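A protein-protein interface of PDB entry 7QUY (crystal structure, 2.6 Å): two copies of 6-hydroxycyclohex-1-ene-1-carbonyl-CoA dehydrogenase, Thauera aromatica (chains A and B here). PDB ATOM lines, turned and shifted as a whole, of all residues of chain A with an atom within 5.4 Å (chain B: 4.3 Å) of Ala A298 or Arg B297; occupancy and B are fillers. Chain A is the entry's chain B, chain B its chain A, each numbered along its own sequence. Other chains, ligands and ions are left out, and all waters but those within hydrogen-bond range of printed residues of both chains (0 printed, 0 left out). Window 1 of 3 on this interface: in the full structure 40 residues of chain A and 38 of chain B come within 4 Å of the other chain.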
ATOM      1  N   LEU A 274      -8.221 -23.807  23.993  1.00  0.00           N
ATOM      2  CA  LEU A 274      -7.805 -24.948  23.138  1.00  0.00           C
ATOM      3  C   LEU A 274      -6.608 -25.619  23.802  1.00  0.00           C
ATOM      4  O   LEU A 274      -5.569 -24.999  23.839  1.00  0.00           O
ATOM      5  CB  LEU A 274      -7.450 -24.451  21.736  1.00  0.00           C
ATOM      6  CG  LEU A 274      -6.819 -25.493  20.820  1.00  0.00           C
ATOM      7  CD1 LEU A 274      -7.738 -26.685  20.635  1.00  0.00           C
ATOM      8  CD2 LEU A 274      -6.477 -24.880  19.483  1.00  0.00           C
ATOM      9  N   ALA A 275      -6.769 -26.833  24.317  1.00  0.00           N
ATOM     10  CA  ALA A 275      -5.684 -27.663  24.884  1.00  0.00           C
ATOM     11  C   ALA A 275      -5.053 -28.478  23.745  1.00  0.00           C
ATOM     12  O   ALA A 275      -5.746 -29.377  23.207  1.00  0.00           O
ATOM     13  CB  ALA A 275      -6.233 -28.552  25.981  1.00  0.00           C
ATOM     14  N   VAL A 276      -3.812 -28.145  23.368  1.00  0.00           N
ATOM     15  CA  VAL A 276      -2.988 -28.869  22.345  1.00  0.00           C
ATOM     16  C   VAL A 276      -2.249 -30.032  23.026  1.00  0.00           C
ATOM     17  O   VAL A 276      -1.237 -29.785  23.721  1.00  0.00           O
ATOM     18  CB  VAL A 276      -1.995 -27.913  21.662  1.00  0.00           C
ATOM     19  CG1 VAL A 276      -1.095 -28.639  20.681  1.00  0.00           C
ATOM     20  CG2 VAL A 276      -2.707 -26.767  20.975  1.00  0.00           C
ATOM     21  N   LEU A 291      -7.614 -15.611  18.606  1.00  0.00           N
ATOM     22  CA  LEU A 291      -7.234 -15.667  20.042  1.00  0.00           C
ATOM     23  C   LEU A 291      -7.512 -14.305  20.680  1.00  0.00           C
ATOM     24  O   LEU A 291      -8.108 -14.295  21.766  1.00  0.00           O
ATOM     25  CB  LEU A 291      -5.766 -16.064  20.184  1.00  0.00           C
ATOM     26  CG  LEU A 291      -5.478 -17.505  20.618  1.00  0.00           C
ATOM     27  CD1 LEU A 291      -6.612 -18.459  20.295  1.00  0.00           C
ATOM     28  CD2 LEU A 291      -4.196 -18.009  19.975  1.00  0.00           C
ATOM     29  N   ALA A 296      -9.433 -15.711  23.830  1.00  0.00           N
ATOM     30  CA  ALA A 296      -9.249 -17.163  24.010  1.00  0.00           C
ATOM     31  C   ALA A 296      -7.764 -17.472  24.206  1.00  0.00           C
ATOM     32  O   ALA A 296      -6.923 -16.562  24.000  1.00  0.00           O
ATOM     33  CB  ALA A 296      -9.794 -17.882  22.808  1.00  0.00           C
ATOM     34  N   ARG A 297      -7.458 -18.724  24.544  1.00  0.00           N
ATOM     35  CA  ARG A 297      -6.074 -19.196  24.767  1.00  0.00           C
ATOM     36  C   ARG A 297      -5.908 -20.606  24.186  1.00  0.00           C
ATOM     37  O   ARG A 297      -6.884 -21.405  24.227  1.00  0.00           O
ATOM     38  CB  ARG A 297      -5.753 -19.169  26.263  1.00  0.00           C
ATOM     39  CG  ARG A 297      -6.721 -19.983  27.093  1.00  0.00           C
ATOM     40  CD  ARG A 297      -6.517 -19.812  28.564  1.00  0.00           C
ATOM     41  NE  ARG A 297      -7.289 -20.836  29.236  1.00  0.00           N
ATOM     42  CZ  ARG A 297      -7.254 -21.077  30.530  1.00  0.00           C
ATOM     43  NH1 ARG A 297      -6.471 -20.343  31.291  1.00  0.00           N
ATOM     44  NH2 ARG A 297      -7.987 -22.055  31.054  1.00  0.00           N
ATOM     45  N   ALA A 298      -4.716 -20.876  23.640  1.00  0.00           N
ATOM     46  CA  ALA A 298      -4.234 -22.215  23.239  1.00  0.00           C
ATOM     47  C   ALA A 298      -3.149 -22.630  24.241  1.00  0.00           C
ATOM     48  O   ALA A 298      -2.151 -21.909  24.353  1.00  0.00           O
ATOM     49  CB  ALA A 298      -3.733 -22.197  21.810  1.00  0.00           C
ATOM     50  N   LEU A 299      -3.370 -23.733  24.960  1.00  0.00           N
ATOM     51  CA  LEU A 299      -2.465 -24.280  26.002  1.00  0.00           C
ATOM     52  C   LEU A 299      -1.858 -25.601  25.526  1.00  0.00           C
ATOM     53  O   LEU A 299      -2.576 -26.595  25.409  1.00  0.00           O
ATOM     54  CB  LEU A 299      -3.252 -24.489  27.295  1.00  0.00           C
ATOM     55  CG  LEU A 299      -3.956 -23.252  27.835  1.00  0.00           C
ATOM     56  CD1 LEU A 299      -4.554 -23.533  29.219  1.00  0.00           C
ATOM     57  CD2 LEU A 299      -3.002 -22.064  27.872  1.00  0.00           C
ATOM     58  N   GLY A 300      -0.553 -25.599  25.288  1.00  0.00           N
ATOM     59  CA  GLY A 300       0.226 -26.838  25.201  1.00  0.00           C
ATOM     60  C   GLY A 300       0.292 -27.557  26.539  1.00  0.00           C
ATOM     61  O   GLY A 300       0.130 -26.916  27.623  1.00  0.00           O
ATOM     62  N   GLN B 167      -1.449 -10.722  32.141  1.00  0.00           N
ATOM     63  CA  GLN B 167      -1.863 -12.091  31.716  1.00  0.00           C
ATOM     64  C   GLN B 167      -0.637 -12.985  31.488  1.00  0.00           C
ATOM     65  O   GLN B 167      -0.708 -14.188  31.789  1.00  0.00           O
ATOM     66  CB  GLN B 167      -2.599 -12.038  30.376  1.00  0.00           C
ATOM     67  CG  GLN B 167      -4.101 -12.238  30.429  1.00  0.00           C
ATOM     68  CD  GLN B 167      -4.611 -12.640  29.063  1.00  0.00           C
ATOM     69  OE1 GLN B 167      -4.130 -12.177  28.025  1.00  0.00           O
ATOM     70  NE2 GLN B 167      -5.567 -13.554  29.050  1.00  0.00           N
ATOM     71  N   ALA B 168       0.424 -12.439  30.887  1.00  0.00           N
ATOM     72  CA  ALA B 168       1.602 -13.208  30.424  1.00  0.00           C
ATOM     73  C   ALA B 168       2.485 -13.548  31.628  1.00  0.00           C
ATOM     74  O   ALA B 168       3.297 -14.456  31.505  1.00  0.00           O
ATOM     75  CB  ALA B 168       2.353 -12.447  29.363  1.00  0.00           C
ATOM     76  N   ALA B 272       7.282 -20.839  27.072  1.00  0.00           N
ATOM     77  CA  ALA B 272       7.047 -19.490  26.506  1.00  0.00           C
ATOM     78  C   ALA B 272       5.556 -19.163  26.543  1.00  0.00           C
ATOM     79  O   ALA B 272       4.766 -20.088  26.457  1.00  0.00           O
ATOM     80  CB  ALA B 272       7.576 -19.401  25.097  1.00  0.00           C
ATOM     81  N   THR B 273       5.215 -17.881  26.665  1.00  0.00           N
ATOM     82  CA  THR B 273       3.852 -17.313  26.496  1.00  0.00           C
ATOM     83  C   THR B 273       3.858 -16.448  25.232  1.00  0.00           C
ATOM     84  O   THR B 273       4.674 -15.502  25.181  1.00  0.00           O
ATOM     85  CB  THR B 273       3.441 -16.452  27.702  1.00  0.00           C
ATOM     86  OG1 THR B 273       3.341 -17.245  28.885  1.00  0.00           O
ATOM     87  CG2 THR B 273       2.117 -15.755  27.486  1.00  0.00           C
ATOM     88  N   LEU B 274       3.008 -16.754  24.250  1.00  0.00           N
ATOM     89  CA  LEU B 274       2.796 -15.856  23.085  1.00  0.00           C
ATOM     90  C   LEU B 274       1.525 -15.052  23.338  1.00  0.00           C
ATOM     91  O   LEU B 274       0.463 -15.653  23.340  1.00  0.00           O
ATOM     92  CB  LEU B 274       2.666 -16.656  21.791  1.00  0.00           C
ATOM     93  CG  LEU B 274       2.311 -15.817  20.563  1.00  0.00           C
ATOM     94  CD1 LEU B 274       3.368 -14.759  20.317  1.00  0.00           C
ATOM     95  CD2 LEU B 274       2.133 -16.678  19.318  1.00  0.00           C
ATOM     96  N   LEU B 291       3.332 -25.866  20.681  1.00  0.00           N
ATOM     97  CA  LEU B 291       2.692 -25.509  21.978  1.00  0.00           C
ATOM     98  C   LEU B 291       2.822 -26.690  22.939  1.00  0.00           C
ATOM     99  O   LEU B 291       3.226 -26.449  24.090  1.00  0.00           O
ATOM    100  CB  LEU B 291       1.227 -25.139  21.750  1.00  0.00           C
ATOM    101  CG  LEU B 291       0.868 -23.652  21.786  1.00  0.00           C
ATOM    102  CD1 LEU B 291       2.040 -22.748  21.464  1.00  0.00           C
ATOM    103  CD2 LEU B 291      -0.282 -23.355  20.846  1.00  0.00           C
ATOM    104  N   ALA B 296       4.140 -24.627  26.021  1.00  0.00           N
ATOM    105  CA  ALA B 296       3.955 -23.172  25.824  1.00  0.00           C
ATOM    106  C   ALA B 296       2.470 -22.871  25.668  1.00  0.00           C
ATOM    107  O   ALA B 296       1.680 -23.819  25.501  1.00  0.00           O
ATOM    108  CB  ALA B 296       4.709 -22.695  24.602  1.00  0.00           C
ATOM    109  N   ARG B 297       2.121 -21.586  25.694  1.00  0.00           N
ATOM    110  CA  ARG B 297       0.718 -21.120  25.621  1.00  0.00           C
ATOM    111  C   ARG B 297       0.642 -19.860  24.756  1.00  0.00           C
ATOM    112  O   ARG B 297       1.614 -19.051  24.793  1.00  0.00           O
ATOM    113  CB  ARG B 297       0.176 -20.893  27.033  1.00  0.00           C
ATOM    114  CG  ARG B 297       1.000 -19.907  27.833  1.00  0.00           C
ATOM    115  CD  ARG B 297       0.500 -19.732  29.244  1.00  0.00           C
ATOM    116  NE  ARG B 297       1.117 -18.524  29.768  1.00  0.00           N
ATOM    117  CZ  ARG B 297       0.860 -17.998  30.950  1.00  0.00           C
ATOM    118  NH1 ARG B 297      -0.027 -18.561  31.739  1.00  0.00           N
ATOM    119  NH2 ARG B 297       1.483 -16.908  31.347  1.00  0.00           N
ATOM    120  N   ALA B 298      -0.449 -19.737  23.984  1.00  0.00           N
ATOM    121  CA  ALA B 298      -0.829 -18.527  23.226  1.00  0.00           C
ATOM    122  C   ALA B 298      -2.052 -17.897  23.903  1.00  0.00           C
ATOM    123  O   ALA B 298      -3.090 -18.579  24.006  1.00  0.00           O
ATOM    124  CB  ALA B 298      -1.102 -18.883  21.786  1.00  0.00           C
ATOM    125  N   LEU B 299      -1.923 -16.647  24.362  1.00  0.00           N
ATOM    126  CA  LEU B 299      -2.979 -15.880  25.074  1.00  0.00           C
ATOM    127  C   LEU B 299      -3.447 -14.696  24.220  1.00  0.00           C
ATOM    128  O   LEU B 299      -2.703 -13.715  24.056  1.00  0.00           O
ATOM    129  CB  LEU B 299      -2.425 -15.391  26.416  1.00  0.00           C
ATOM    130  CG  LEU B 299      -1.860 -16.464  27.326  1.00  0.00           C
ATOM    131  CD1 LEU B 299      -1.537 -15.908  28.688  1.00  0.00           C
ATOM    132  CD2 LEU B 299      -2.817 -17.617  27.471  1.00  0.00           C
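O of Leu B274 sits at hydrogen-bond distance from N of Leu B299 (2.8 Å).
The backbone NH (N) of Ala B296 sits at hydrogen-bond distance from the backbone carbonyl oxygen (O) of Leu B291, 2.8 Å away.
O of Arg A297 lies within hydrogen-bond range of N of Leu A274 (2.8 Å).
N of Arg B297 lies within hydrogen-bond range of O of Ala B272 (3.1 Å).
O of Leu A274 lies within hydrogen-bond range of N of Leu A299, at 2.8 Å.
The backbone NH (N) of Ala A296 sits at hydrogen-bond distance from the backbone carbonyl oxygen (O) of Leu A291, 2.8 Å away.
Of the 10 printed residues of chain B, 5 touch a printed residue of chain A.
Hydrophobic or aromatic side chains of chain B within 4 Å of the printed part of chain A: Leu B291, Ala B298 and Leu B299.
Of the 9 printed residues of chain A, 6 touch a printed residue of chain B.
Among the printed residues, no Asp or Glu carboxylate lies within 4 Å of a Lys or Arg side-chain nitrogen of the other chain.
Leu A291 touches Ala B298, and with the chains exchanged Ala A298 touches Leu B291.
Arg A297 touches Ala B298, and with the chains exchanged Ala A298 touches Arg B297.
Arg A297 touches Leu B299, and with the chains exchanged Leu A299 touches Arg B297.
Ala A298 touches its own counterpart, Ala B298.
6 positions are printed for both chains.
Among the printed residues, merely in contact across the chains: Arg A297 with Ala B298 (3.1 Å), Gly A300 with Leu B291 (3.2 Å), Ala A298 with Arg B297 (3.2 Å), Leu A299 with Arg B297 (3.5 Å), Arg A297 with Leu B299 (3.5 Å), Leu A291 with Ala B298 (3.7 Å), Ala A298 with Leu B291 (3.8 Å), Ala A296 with Leu B299 (3.95 Å) and Leu A299 with Ala B296 (3.96 Å).
O of Ala B296 lies within hydrogen-bond range of N of Gly A300 (2.9 Å).
N of Ala B298 is in hydrogen-bond range of O of Ala A298 (2.8 Å).
Of chain B, only Leu B291 (3.8 Å), Arg B297 (3.2 Å) and Ala B298 (2.8 Å) come within 4 Å of Ala A298.
Of chain A, only Ala A298 (3.2 Å) and Leu A299 (3.5 Å) come within 4 Å of Arg B297.
Of the printed residues of chain B, Leu A299 touches Ala B296 (3.96 Å) and Arg B297 (3.5 Å).
Of the printed residues of chain A, Leu B291 touches Ala A298 (3.8 Å) and Gly A300 (3.2 Å).
Of the printed residues of chain B, Arg A297 touches Ala B298 (3.1 Å) and Leu B299 (3.5 Å).
Ala B168 touches none of the printed residues of chain A.
The nearest printed residue of chain B that does not touch Leu A299 is Leu B299 (4.5 Å).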
